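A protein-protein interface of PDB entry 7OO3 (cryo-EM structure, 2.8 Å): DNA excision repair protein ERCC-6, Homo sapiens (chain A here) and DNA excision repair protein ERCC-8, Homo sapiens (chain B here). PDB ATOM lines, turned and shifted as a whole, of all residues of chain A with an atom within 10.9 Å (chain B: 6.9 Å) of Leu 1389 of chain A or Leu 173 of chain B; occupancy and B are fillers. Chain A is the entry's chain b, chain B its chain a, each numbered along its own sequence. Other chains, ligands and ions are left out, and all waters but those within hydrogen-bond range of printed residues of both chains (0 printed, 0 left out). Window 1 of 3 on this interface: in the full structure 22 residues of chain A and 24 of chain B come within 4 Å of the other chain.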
ATOM      1  N   LYS A 729      14.184  11.148 -10.979  1.00  0.00           N
ATOM      2  CA  LYS A 729      13.736  10.909 -12.349  1.00  0.00           C
ATOM      3  C   LYS A 729      12.533  11.776 -12.697  1.00  0.00           C
ATOM      4  O   LYS A 729      12.470  12.371 -13.782  1.00  0.00           O
ATOM      5  CB  LYS A 729      13.393   9.432 -12.532  1.00  0.00           C
ATOM      6  CG  LYS A 729      13.008   9.060 -13.957  1.00  0.00           C
ATOM      7  CD  LYS A 729      11.506   8.833 -14.103  1.00  0.00           C
ATOM      8  CE  LYS A 729      11.174   8.080 -15.382  1.00  0.00           C
ATOM      9  NZ  LYS A 729       9.782   7.554 -15.368  1.00  0.00           N
ATOM     10  N   VAL A 733      12.040  14.699 -15.560  1.00  0.00           N
ATOM     11  CA  VAL A 733      10.962  14.710 -16.547  1.00  0.00           C
ATOM     12  C   VAL A 733      10.201  16.029 -16.502  1.00  0.00           C
ATOM     13  O   VAL A 733       9.855  16.604 -17.540  1.00  0.00           O
ATOM     14  CB  VAL A 733      10.029  13.504 -16.332  1.00  0.00           C
ATOM     15  CG1 VAL A 733       8.763  13.648 -17.162  1.00  0.00           C
ATOM     16  CG2 VAL A 733      10.750  12.216 -16.696  1.00  0.00           C
ATOM     17  N   ASP A 736      12.574  18.865 -18.124  1.00  0.00           N
ATOM     18  CA  ASP A 736      12.679  18.917 -19.578  1.00  0.00           C
ATOM     19  C   ASP A 736      11.316  19.141 -20.228  1.00  0.00           C
ATOM     20  O   ASP A 736      11.251  19.692 -21.332  1.00  0.00           O
ATOM     21  CB  ASP A 736      13.383  17.667 -20.117  1.00  0.00           C
ATOM     22  CG  ASP A 736      12.638  16.400 -19.833  1.00  0.00           C
ATOM     23  OD1 ASP A 736      11.590  16.457 -19.196  1.00  0.00           O
ATOM     24  OD2 ASP A 736      13.131  15.325 -20.198  1.00  0.00           O
ATOM     25  N   THR A 737      10.218  18.732 -19.578  1.00  0.00           N
ATOM     26  CA  THR A 737       8.903  19.063 -20.115  1.00  0.00           C
ATOM     27  C   THR A 737       8.670  20.570 -20.104  1.00  0.00           C
ATOM     28  O   THR A 737       8.114  21.122 -21.060  1.00  0.00           O
ATOM     29  CB  THR A 737       7.810  18.339 -19.328  1.00  0.00           C
ATOM     30  OG1 THR A 737       8.013  16.924 -19.425  1.00  0.00           O
ATOM     31  CG2 THR A 737       6.416  18.676 -19.869  1.00  0.00           C
ATOM     32  N   PRO A1383      18.035  13.514 -37.581  1.00  0.00           N
ATOM     33  CA  PRO A1383      17.199  12.579 -36.821  1.00  0.00           C
ATOM     34  C   PRO A1383      17.996  11.729 -35.840  1.00  0.00           C
ATOM     35  O   PRO A1383      19.113  11.318 -36.150  1.00  0.00           O
ATOM     36  CB  PRO A1383      16.578  11.704 -37.909  1.00  0.00           C
ATOM     37  CG  PRO A1383      17.565  11.723 -39.023  1.00  0.00           C
ATOM     38  CD  PRO A1383      18.325  13.022 -38.940  1.00  0.00           C
ATOM     39  N   LEU A1384      17.423  11.475 -34.667  1.00  0.00           N
ATOM     40  CA  LEU A1384      18.060  10.590 -33.704  1.00  0.00           C
ATOM     41  C   LEU A1384      18.156   9.190 -34.293  1.00  0.00           C
ATOM     42  O   LEU A1384      17.167   8.654 -34.801  1.00  0.00           O
ATOM     43  CB  LEU A1384      17.262  10.566 -32.401  1.00  0.00           C
ATOM     44  CG  LEU A1384      17.575  11.656 -31.375  1.00  0.00           C
ATOM     45  CD1 LEU A1384      17.428  13.050 -31.972  1.00  0.00           C
ATOM     46  CD2 LEU A1384      16.676  11.502 -30.159  1.00  0.00           C
ATOM     47  N   ALA A1385      19.344   8.597 -34.231  1.00  0.00           N
ATOM     48  CA  ALA A1385      19.582   7.320 -34.901  1.00  0.00           C
ATOM     49  C   ALA A1385      19.316   6.134 -33.980  1.00  0.00           C
ATOM     50  O   ALA A1385      20.111   5.200 -33.897  1.00  0.00           O
ATOM     51  CB  ALA A1385      21.008   7.282 -35.436  1.00  0.00           C
ATOM     52  N   SER A1386      18.179   6.167 -33.283  1.00  0.00           N
ATOM     53  CA  SER A1386      17.595   5.009 -32.597  1.00  0.00           C
ATOM     54  C   SER A1386      18.566   4.309 -31.639  1.00  0.00           C
ATOM     55  O   SER A1386      18.298   3.182 -31.214  1.00  0.00           O
ATOM     56  CB  SER A1386      17.057   4.002 -33.620  1.00  0.00           C
ATOM     57  OG  SER A1386      16.667   2.772 -33.028  1.00  0.00           O
ATOM     58  N   SER A1387      19.687   4.931 -31.287  1.00  0.00           N
ATOM     59  CA  SER A1387      20.577   4.437 -30.244  1.00  0.00           C
ATOM     60  C   SER A1387      20.813   5.470 -29.162  1.00  0.00           C
ATOM     61  O   SER A1387      20.819   5.128 -27.978  1.00  0.00           O
ATOM     62  CB  SER A1387      21.921   4.008 -30.847  1.00  0.00           C
ATOM     63  OG  SER A1387      21.751   2.911 -31.727  1.00  0.00           O
ATOM     64  N   SER A1388      21.001   6.733 -29.543  1.00  0.00           N
ATOM     65  CA  SER A1388      20.901   7.810 -28.569  1.00  0.00           C
ATOM     66  C   SER A1388      19.508   7.839 -27.960  1.00  0.00           C
ATOM     67  O   SER A1388      19.349   8.068 -26.756  1.00  0.00           O
ATOM     68  CB  SER A1388      21.233   9.145 -29.233  1.00  0.00           C
ATOM     69  OG  SER A1388      20.350   9.410 -30.308  1.00  0.00           O
ATOM     70  N   LEU A1389      18.487   7.591 -28.780  1.00  0.00           N
ATOM     71  CA  LEU A1389      17.121   7.521 -28.277  1.00  0.00           C
ATOM     72  C   LEU A1389      16.946   6.345 -27.321  1.00  0.00           C
ATOM     73  O   LEU A1389      16.425   6.507 -26.208  1.00  0.00           O
ATOM     74  CB  LEU A1389      16.168   7.405 -29.464  1.00  0.00           C
ATOM     75  CG  LEU A1389      14.668   7.531 -29.228  1.00  0.00           C
ATOM     76  CD1 LEU A1389      14.297   8.907 -28.698  1.00  0.00           C
ATOM     77  CD2 LEU A1389      13.909   7.211 -30.505  1.00  0.00           C
ATOM     78  N   LEU A1390      17.437   5.167 -27.708  1.00  0.00           N
ATOM     79  CA  LEU A1390      17.360   4.013 -26.825  1.00  0.00           C
ATOM     80  C   LEU A1390      18.275   4.162 -25.623  1.00  0.00           C
ATOM     81  O   LEU A1390      17.918   3.729 -24.522  1.00  0.00           O
ATOM     82  CB  LEU A1390      17.729   2.734 -27.579  1.00  0.00           C
ATOM     83  CG  LEU A1390      16.683   2.025 -28.435  1.00  0.00           C
ATOM     84  CD1 LEU A1390      17.332   0.900 -29.205  1.00  0.00           C
ATOM     85  CD2 LEU A1390      15.592   1.468 -27.549  1.00  0.00           C
ATOM     86  N   ALA A1391      19.448   4.769 -25.814  1.00  0.00           N
ATOM     87  CA  ALA A1391      20.353   4.969 -24.690  1.00  0.00           C
ATOM     88  C   ALA A1391      19.725   5.885 -23.652  1.00  0.00           C
ATOM     89  O   ALA A1391      19.776   5.598 -22.452  1.00  0.00           O
ATOM     90  CB  ALA A1391      21.680   5.548 -25.180  1.00  0.00           C
ATOM     91  N   LYS A1392      19.084   6.965 -24.100  1.00  0.00           N
ATOM     92  CA  LYS A1392      18.413   7.861 -23.171  1.00  0.00           C
ATOM     93  C   LYS A1392      17.231   7.181 -22.497  1.00  0.00           C
ATOM     94  O   LYS A1392      17.014   7.376 -21.294  1.00  0.00           O
ATOM     95  CB  LYS A1392      17.970   9.125 -23.906  1.00  0.00           C
ATOM     96  CG  LYS A1392      19.126  10.052 -24.261  1.00  0.00           C
ATOM     97  CD  LYS A1392      18.670  11.256 -25.067  1.00  0.00           C
ATOM     98  CE  LYS A1392      19.843  12.160 -25.426  1.00  0.00           C
ATOM     99  NZ  LYS A1392      19.410  13.437 -26.060  1.00  0.00           N
ATOM    100  N   MET A1393      16.484   6.346 -23.228  1.00  0.00           N
ATOM    101  CA  MET A1393      15.355   5.675 -22.593  1.00  0.00           C
ATOM    102  C   MET A1393      15.818   4.709 -21.512  1.00  0.00           C
ATOM    103  O   MET A1393      15.292   4.730 -20.391  1.00  0.00           O
ATOM    104  CB  MET A1393      14.515   4.929 -23.633  1.00  0.00           C
ATOM    105  CG  MET A1393      13.501   5.799 -24.352  1.00  0.00           C
ATOM    106  SD  MET A1393      12.337   4.890 -25.373  1.00  0.00           S
ATOM    107  CE  MET A1393      12.827   5.434 -26.990  1.00  0.00           C
ATOM    108  N   ARG A1394      16.830   3.892 -21.803  1.00  0.00           N
ATOM    109  CA  ARG A1394      17.294   2.948 -20.794  1.00  0.00           C
ATOM    110  C   ARG A1394      17.986   3.655 -19.639  1.00  0.00           C
ATOM    111  O   ARG A1394      17.864   3.210 -18.488  1.00  0.00           O
ATOM    112  CB  ARG A1394      18.235   1.922 -21.427  1.00  0.00           C
ATOM    113  CG  ARG A1394      19.557   2.492 -21.940  1.00  0.00           C
ATOM    114  CD  ARG A1394      20.521   1.397 -22.384  1.00  0.00           C
ATOM    115  NE  ARG A1394      19.979   0.605 -23.492  1.00  0.00           N
ATOM    116  CZ  ARG A1394      19.357  -0.568 -23.377  1.00  0.00           C
ATOM    117  NH1 ARG A1394      19.168  -1.137 -22.190  1.00  0.00           N
ATOM    118  NH2 ARG A1394      18.912  -1.181 -24.468  1.00  0.00           N
ATOM    119  N   ALA A1395      18.661   4.774 -19.914  1.00  0.00           N
ATOM    120  CA  ALA A1395      19.272   5.549 -18.846  1.00  0.00           C
ATOM    121  C   ALA A1395      18.210   6.057 -17.891  1.00  0.00           C
ATOM    122  O   ALA A1395      18.302   5.845 -16.678  1.00  0.00           O
ATOM    123  CB  ALA A1395      20.073   6.708 -19.437  1.00  0.00           C
ATOM    124  N   ARG A1396      17.169   6.695 -18.425  1.00  0.00           N
ATOM    125  CA  ARG A1396      16.131   7.215 -17.549  1.00  0.00           C
ATOM    126  C   ARG A1396      15.415   6.094 -16.817  1.00  0.00           C
ATOM    127  O   ARG A1396      14.971   6.287 -15.680  1.00  0.00           O
ATOM    128  CB  ARG A1396      15.123   8.037 -18.343  1.00  0.00           C
ATOM    129  CG  ARG A1396      15.667   9.332 -18.898  1.00  0.00           C
ATOM    130  CD  ARG A1396      14.558  10.076 -19.592  1.00  0.00           C
ATOM    131  NE  ARG A1396      14.134   9.395 -20.815  1.00  0.00           N
ATOM    132  CZ  ARG A1396      12.953   8.810 -21.010  1.00  0.00           C
ATOM    133  NH1 ARG A1396      12.022   8.768 -20.061  1.00  0.00           N
ATOM    134  NH2 ARG A1396      12.697   8.251 -22.177  1.00  0.00           N
ATOM    135  N   ASN A1397      15.302   4.917 -17.435  1.00  0.00           N
ATOM    136  CA  ASN A1397      14.538   3.850 -16.800  1.00  0.00           C
ATOM    137  C   ASN A1397      15.317   3.141 -15.698  1.00  0.00           C
ATOM    138  O   ASN A1397      14.700   2.654 -14.743  1.00  0.00           O
ATOM    139  CB  ASN A1397      14.062   2.843 -17.846  1.00  0.00           C
ATOM    140  CG  ASN A1397      12.729   3.234 -18.461  1.00  0.00           C
ATOM    141  OD1 ASN A1397      12.454   4.416 -18.669  1.00  0.00           O
ATOM    142  ND2 ASN A1397      11.883   2.246 -18.730  1.00  0.00           N
ATOM    143  N   HIS A1398      16.653   3.066 -15.776  1.00  0.00           N
ATOM    144  CA  HIS A1398      17.373   2.419 -14.677  1.00  0.00           C
ATOM    145  C   HIS A1398      17.289   3.221 -13.383  1.00  0.00           C
ATOM    146  O   HIS A1398      17.393   2.642 -12.297  1.00  0.00           O
ATOM    147  CB  HIS A1398      18.840   2.173 -15.027  1.00  0.00           C
ATOM    148  CG  HIS A1398      19.051   1.174 -16.118  1.00  0.00           C
ATOM    149  ND1 HIS A1398      19.085   1.514 -17.452  1.00  0.00           N
ATOM    150  CD2 HIS A1398      19.230  -0.168 -16.069  1.00  0.00           C
ATOM    151  CE1 HIS A1398      19.281   0.426 -18.179  1.00  0.00           C
ATOM    152  NE2 HIS A1398      19.375  -0.608 -17.363  1.00  0.00           N
ATOM    153  N   TYR B 108      10.067   2.310 -35.676  1.00  0.00           N
ATOM    154  CA  TYR B 108      10.587   3.650 -35.534  1.00  0.00           C
ATOM    155  C   TYR B 108      10.956   4.140 -36.924  1.00  0.00           C
ATOM    156  O   TYR B 108      11.737   3.470 -37.609  1.00  0.00           O
ATOM    157  CB  TYR B 108      11.810   3.665 -34.637  1.00  0.00           C
ATOM    158  CG  TYR B 108      12.425   5.030 -34.461  1.00  0.00           C
ATOM    159  CD1 TYR B 108      11.696   6.071 -33.911  1.00  0.00           C
ATOM    160  CD2 TYR B 108      13.732   5.276 -34.839  1.00  0.00           C
ATOM    161  CE1 TYR B 108      12.252   7.320 -33.748  1.00  0.00           C
ATOM    162  CE2 TYR B 108      14.298   6.521 -34.679  1.00  0.00           C
ATOM    163  CZ  TYR B 108      13.554   7.541 -34.133  1.00  0.00           C
ATOM    164  OH  TYR B 108      14.112   8.787 -33.970  1.00  0.00           O
ATOM    165  N   MET B 114      14.463   0.264 -33.496  1.00  0.00           N
ATOM    166  CA  MET B 114      13.478   0.506 -32.453  1.00  0.00           C
ATOM    167  C   MET B 114      12.080   0.403 -33.042  1.00  0.00           C
ATOM    168  O   MET B 114      11.858   0.793 -34.190  1.00  0.00           O
ATOM    169  CB  MET B 114      13.700   1.891 -31.850  1.00  0.00           C
ATOM    170  CG  MET B 114      13.292   2.057 -30.419  1.00  0.00           C
ATOM    171  SD  MET B 114      12.715   3.728 -30.097  1.00  0.00           S
ATOM    172  CE  MET B 114      11.069   3.630 -30.773  1.00  0.00           C
ATOM    173  N   THR B 116       7.686   0.551 -31.610  1.00  0.00           N
ATOM    174  CA  THR B 116       6.784   0.771 -30.491  1.00  0.00           C
ATOM    175  C   THR B 116       5.461   0.080 -30.777  1.00  0.00           C
ATOM    176  O   THR B 116       5.029  -0.016 -31.927  1.00  0.00           O
ATOM    177  CB  THR B 116       6.564   2.272 -30.219  1.00  0.00           C
ATOM    178  OG1 THR B 116       5.764   2.842 -31.254  1.00  0.00           O
ATOM    179  CG2 THR B 116       7.876   3.016 -30.163  1.00  0.00           C
ATOM    180  N   LEU B 124       1.927   1.566 -23.939  1.00  0.00           N
ATOM    181  CA  LEU B 124       2.692   1.751 -25.165  1.00  0.00           C
ATOM    182  C   LEU B 124       4.134   1.409 -24.819  1.00  0.00           C
ATOM    183  O   LEU B 124       4.805   2.174 -24.121  1.00  0.00           O
ATOM    184  CB  LEU B 124       2.563   3.183 -25.680  1.00  0.00           C
ATOM    185  CG  LEU B 124       3.593   3.707 -26.681  1.00  0.00           C
ATOM    186  CD1 LEU B 124       3.563   2.900 -27.957  1.00  0.00           C
ATOM    187  CD2 LEU B 124       3.342   5.168 -26.969  1.00  0.00           C
ATOM    188  N   VAL B 126       8.056   0.631 -25.867  1.00  0.00           N
ATOM    189  CA  VAL B 126       9.109   0.863 -26.845  1.00  0.00           C
ATOM    190  C   VAL B 126      10.090  -0.295 -26.744  1.00  0.00           C
ATOM    191  O   VAL B 126      10.644  -0.552 -25.670  1.00  0.00           O
ATOM    192  CB  VAL B 126       9.817   2.204 -26.590  1.00  0.00           C
ATOM    193  CG1 VAL B 126      10.887   2.443 -27.624  1.00  0.00           C
ATOM    194  CG2 VAL B 126       8.818   3.352 -26.554  1.00  0.00           C
ATOM    195  N   ALA B 135      12.646  -0.748 -23.917  1.00  0.00           N
ATOM    196  CA  ALA B 135      13.452   0.381 -23.474  1.00  0.00           C
ATOM    197  C   ALA B 135      12.650   1.395 -22.673  1.00  0.00           C
ATOM    198  O   ALA B 135      13.236   2.149 -21.890  1.00  0.00           O
ATOM    199  CB  ALA B 135      14.087   1.080 -24.675  1.00  0.00           C
ATOM    200  N   ASP B 136      11.335   1.434 -22.859  1.00  0.00           N
ATOM    201  CA  ASP B 136      10.470   2.337 -22.119  1.00  0.00           C
ATOM    202  C   ASP B 136       9.054   1.793 -22.183  1.00  0.00           C
ATOM    203  O   ASP B 136       8.698   1.050 -23.097  1.00  0.00           O
ATOM    204  CB  ASP B 136      10.530   3.762 -22.671  1.00  0.00           C
ATOM    205  CG  ASP B 136      10.043   4.796 -21.677  1.00  0.00           C
ATOM    206  OD1 ASP B 136       9.529   4.405 -20.608  1.00  0.00           O
ATOM    207  OD2 ASP B 136      10.170   6.003 -21.968  1.00  0.00           O
ATOM    208  N   PHE B 138       5.019   3.362 -21.502  1.00  0.00           N
ATOM    209  CA  PHE B 138       4.124   4.471 -21.202  1.00  0.00           C
ATOM    210  C   PHE B 138       2.794   3.865 -20.786  1.00  0.00           C
ATOM    211  O   PHE B 138       2.069   3.314 -21.615  1.00  0.00           O
ATOM    212  CB  PHE B 138       3.952   5.388 -22.403  1.00  0.00           C
ATOM    213  CG  PHE B 138       5.208   6.083 -22.818  1.00  0.00           C
ATOM    214  CD1 PHE B 138       6.098   5.469 -23.674  1.00  0.00           C
ATOM    215  CD2 PHE B 138       5.497   7.349 -22.354  1.00  0.00           C
ATOM    216  CE1 PHE B 138       7.250   6.105 -24.060  1.00  0.00           C
ATOM    217  CE2 PHE B 138       6.647   7.987 -22.736  1.00  0.00           C
ATOM    218  CZ  PHE B 138       7.525   7.364 -23.591  1.00  0.00           C
ATOM    219  N   MET B 149       3.748   7.321 -34.655  1.00  0.00           N
ATOM    220  CA  MET B 149       4.898   8.209 -34.684  1.00  0.00           C
ATOM    221  C   MET B 149       4.941   8.919 -36.025  1.00  0.00           C
ATOM    222  O   MET B 149       4.610   8.332 -37.056  1.00  0.00           O
ATOM    223  CB  MET B 149       6.194   7.430 -34.479  1.00  0.00           C
ATOM    224  CG  MET B 149       6.485   7.097 -33.045  1.00  0.00           C
ATOM    225  SD  MET B 149       8.008   6.170 -32.821  1.00  0.00           S
ATOM    226  CE  MET B 149       7.547   4.585 -33.508  1.00  0.00           C
ATOM    227  N   CYS B 157       9.966  13.571 -31.707  1.00  0.00           N
ATOM    228  CA  CYS B 157       9.731  12.135 -31.779  1.00  0.00           C
ATOM    229  C   CYS B 157       8.554  11.808 -30.865  1.00  0.00           C
ATOM    230  O   CYS B 157       8.633  10.929 -30.003  1.00  0.00           O
ATOM    231  CB  CYS B 157      11.004  11.370 -31.410  1.00  0.00           C
ATOM    232  SG  CYS B 157      10.843   9.572 -31.332  1.00  0.00           S
ATOM    233  N   LEU B 158       7.470  12.559 -31.022  1.00  0.00           N
ATOM    234  CA  LEU B 158       6.250  12.326 -30.267  1.00  0.00           C
ATOM    235  C   LEU B 158       5.484  11.141 -30.832  1.00  0.00           C
ATOM    236  O   LEU B 158       5.462  10.915 -32.044  1.00  0.00           O
ATOM    237  CB  LEU B 158       5.351  13.562 -30.294  1.00  0.00           C
ATOM    238  CG  LEU B 158       5.978  14.931 -30.038  1.00  0.00           C
ATOM    239  CD1 LEU B 158       5.013  16.026 -30.440  1.00  0.00           C
ATOM    240  CD2 LEU B 158       6.354  15.067 -28.578  1.00  0.00           C
ATOM    241  N   VAL B 159       4.854  10.390 -29.939  1.00  0.00           N
ATOM    242  CA  VAL B 159       3.900   9.350 -30.289  1.00  0.00           C
ATOM    243  C   VAL B 159       2.532   9.889 -29.915  1.00  0.00           C
ATOM    244  O   VAL B 159       2.286  10.216 -28.748  1.00  0.00           O
ATOM    245  CB  VAL B 159       4.176   8.029 -29.553  1.00  0.00           C
ATOM    246  CG1 VAL B 159       3.364   6.904 -30.176  1.00  0.00           C
ATOM    247  CG2 VAL B 159       5.657   7.693 -29.528  1.00  0.00           C
ATOM    248  N   CYS B 171       3.244  11.461 -26.278  1.00  0.00           N
ATOM    249  CA  CYS B 171       4.344  10.930 -25.479  1.00  0.00           C
ATOM    250  C   CYS B 171       5.652  11.206 -26.203  1.00  0.00           C
ATOM    251  O   CYS B 171       5.841  10.750 -27.330  1.00  0.00           O
ATOM    252  CB  CYS B 171       4.171   9.430 -25.254  1.00  0.00           C
ATOM    253  SG  CYS B 171       2.529   8.949 -24.711  1.00  0.00           S
ATOM    254  N   ASP B 172       6.565  11.912 -25.550  1.00  0.00           N
ATOM    255  CA  ASP B 172       7.853  12.238 -26.149  1.00  0.00           C
ATOM    256  C   ASP B 172       8.828  11.109 -25.843  1.00  0.00           C
ATOM    257  O   ASP B 172       9.166  10.873 -24.682  1.00  0.00           O
ATOM    258  CB  ASP B 172       8.365  13.573 -25.617  1.00  0.00           C
ATOM    259  CG  ASP B 172       9.224  14.314 -26.624  1.00  0.00           C
ATOM    260  OD1 ASP B 172       9.854  13.652 -27.473  1.00  0.00           O
ATOM    261  OD2 ASP B 172       9.266  15.561 -26.565  1.00  0.00           O
ATOM    262  N   LEU B 173       9.266  10.394 -26.879  1.00  0.00           N
ATOM    263  CA  LEU B 173      10.256   9.340 -26.673  1.00  0.00           C
ATOM    264  C   LEU B 173      11.610   9.937 -26.320  1.00  0.00           C
ATOM    265  O   LEU B 173      12.308   9.434 -25.433  1.00  0.00           O
ATOM    266  CB  LEU B 173      10.357   8.459 -27.911  1.00  0.00           C
ATOM    267  CG  LEU B 173       9.130   7.653 -28.343  1.00  0.00           C
ATOM    268  CD1 LEU B 173       9.560   6.567 -29.298  1.00  0.00           C
ATOM    269  CD2 LEU B 173       8.373   7.044 -27.169  1.00  0.00           C
ATOM    270  N   LYS B 174      12.012  10.997 -27.022  1.00  0.00           N
ATOM    271  CA  LYS B 174      13.028  11.880 -26.473  1.00  0.00           C
ATOM    272  C   LYS B 174      12.508  12.303 -25.113  1.00  0.00           C
ATOM    273  O   LYS B 174      11.292  12.429 -24.946  1.00  0.00           O
ATOM    274  CB  LYS B 174      13.287  13.086 -27.377  1.00  0.00           C
ATOM    275  CG  LYS B 174      13.981  12.744 -28.686  1.00  0.00           C
ATOM    276  CD  LYS B 174      14.185  13.981 -29.544  1.00  0.00           C
ATOM    277  CE  LYS B 174      14.899  13.643 -30.842  1.00  0.00           C
ATOM    278  NZ  LYS B 174      15.084  14.843 -31.703  1.00  0.00           N
ATOM    279  N   SER B 175      13.410  12.632 -24.189  1.00  0.00           N
ATOM    280  CA  SER B 175      13.230  12.399 -22.757  1.00  0.00           C
ATOM    281  C   SER B 175      11.779  12.501 -22.284  1.00  0.00           C
ATOM    282  O   SER B 175      11.082  13.483 -22.553  1.00  0.00           O
ATOM    283  CB  SER B 175      14.132  13.372 -22.000  1.00  0.00           C
ATOM    284  OG  SER B 175      14.119  13.122 -20.605  1.00  0.00           O
ATOM    285  N   GLY B 176      11.343  11.467 -21.565  1.00  0.00           N
ATOM    286  CA  GLY B 176       9.962  11.021 -21.490  1.00  0.00           C
ATOM    287  C   GLY B 176       8.930  11.933 -20.866  1.00  0.00           C
ATOM    288  O   GLY B 176       8.912  12.106 -19.646  1.00  0.00           O
ATOM    289  N   SER B 177       8.043  12.492 -21.689  1.00  0.00           N
ATOM    290  CA  SER B 177       6.973  13.378 -21.230  1.00  0.00           C
ATOM    291  C   SER B 177       5.666  12.922 -21.869  1.00  0.00           C
ATOM    292  O   SER B 177       5.398  13.242 -23.031  1.00  0.00           O
ATOM    293  CB  SER B 177       7.282  14.829 -21.573  1.00  0.00           C
ATOM    294  OG  SER B 177       7.295  15.028 -22.975  1.00  0.00           O
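OH of Tyr 108 of chain B is in hydrogen-bond range of O of Leu 1384 of chain A (3.2 Å). The side-chain hydroxyl (OG) of Ser 1386 of chain A sits close to the backbone NH (N) of Met 114 of chain B. The side-chain amide nitrogen (ND2) of Asn 1397 of chain A is in hydrogen-bond range of the backbone carbonyl oxygen (O) of Ala 135 of chain B, 3.4 Å away. The side-chain carboxylate (OD2) of Asp 136 of chain B is in salt-bridge range of the guanidinium group (NH2) of Arg 1396 of chain A (3.4 Å). O of Leu 173 of chain B sits at hydrogen-bond distance from NH2 of Arg 1396 of chain A (3.5 Å). The side-chain carboxylate of Asp 736 of chain A is in hydrogen-bond range of the side-chain hydroxyl of Ser 175 of chain B (2.4 Å). The backbone NH (N) of Gly 176 of chain B sits close to the guanidinium group (NH1) of Arg 1396 of chain A (3.2 Å).
N of Tyr 108 of chain B sits at hydrogen-bond distance from O of Met 114 of chain B (2.8 Å). O of Val 126 of chain B sits at hydrogen-bond distance from N of Ala 135 of chain B (2.7 Å). N of Val 126 of chain B lies within hydrogen-bond range of O of Asp 136 of chain B (2.9 Å). N of Asp 172 of chain B lies within hydrogen-bond range of O of Ser 177 of chain B (3.1 Å). O of Val 733 of chain A sits close to OD1 of Asp 736 of chain A (2.4 Å). The backbone carbonyl oxygen (O) of Met 1393 of chain A sits close to the side-chain amide oxygen (OD1) of Asn 1397 of chain A, 3.3 Å away.
Among the printed residues, pairs that only touch across the chains: Leu 1384 of chain A with Lys 174 of chain B, Val 733 of chain A with Gly 176 of chain B, Thr 737 of chain A with Ser 177 of chain B, Arg 1396 of chain A with Ser 175 of chain B, Leu 1390 of chain A with Ala 135 of chain B, Met 1393 of chain A with Asp 136 of chain B, Asn 1397 of chain A with Asp 136 of chain B, Leu 1389 of chain A with Lys 174 of chain B, Met 1393 of chain A with Ala 135 of chain B, Met 1393 of chain A with Met 114 of chain B, Met 1393 of chain A with Val 126 of chain B, Leu 1389 of chain A with Tyr 108 of chain B, Leu 1389 of chain A with Met 114 of chain B, Leu 1390 of chain A with Met 114 of chain B, Leu 1389 of chain A with Leu 173 of chain B, Ser 1386 of chain A with Tyr 108 of chain B, Leu 1389 of chain A with Cys 157 of chain B, Met 1393 of chain A with Leu 173 of chain B and Arg 1394 of chain A with Ala 135 of chain B.
Printed residues of chain B within 4 Å of Thr 737 of chain A: Ser 177. Leu 1389 of chain A touches just these residues of chain B: Tyr 108 (3.6 Å), Met 114 (3.7 Å), Cys 157 (3.96 Å), Leu 173 (3.7 Å) and Lys 174 (3.5 Å). Of the printed residues of chain B, Leu 1390 of chain A touches Met 114 and Ala 135. Ala 1391 of chain A touches none of the printed residues of chain B. Cys 171 of chain B touches none of the printed residues of chain A. No residue of chain A comes within 4 Å of Asp 172 of chain B. Lys 174 of chain B touches two residues of chain A. Of chain A, only Asp 736 and Arg 1396 come within 4 Å of Ser 175 of chain B. Printed residues of chain A within 4 Å of Ser 177 of chain B: Thr 737. The nearest residue of chain B that does not touch Leu 1389 of chain A is Ser 175 of chain B (5.9 Å). The nearest residue of chain A that does not touch Leu 173 of chain B is Lys 1392 of chain A (5.9 Å).
Hydrophobic or aromatic side chains of chain A that line the printed part of chain B: Val 733, Leu 1384, Leu 1389, Leu 1390 and Met 1393. Of the 19 printed residues of chain B, 11 touch a printed residue of chain A. Along chain B the printed residues that touch a printed residue of chain A span positions 108 to 177. Among the printed residues, 26 pairs touch across the chains.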
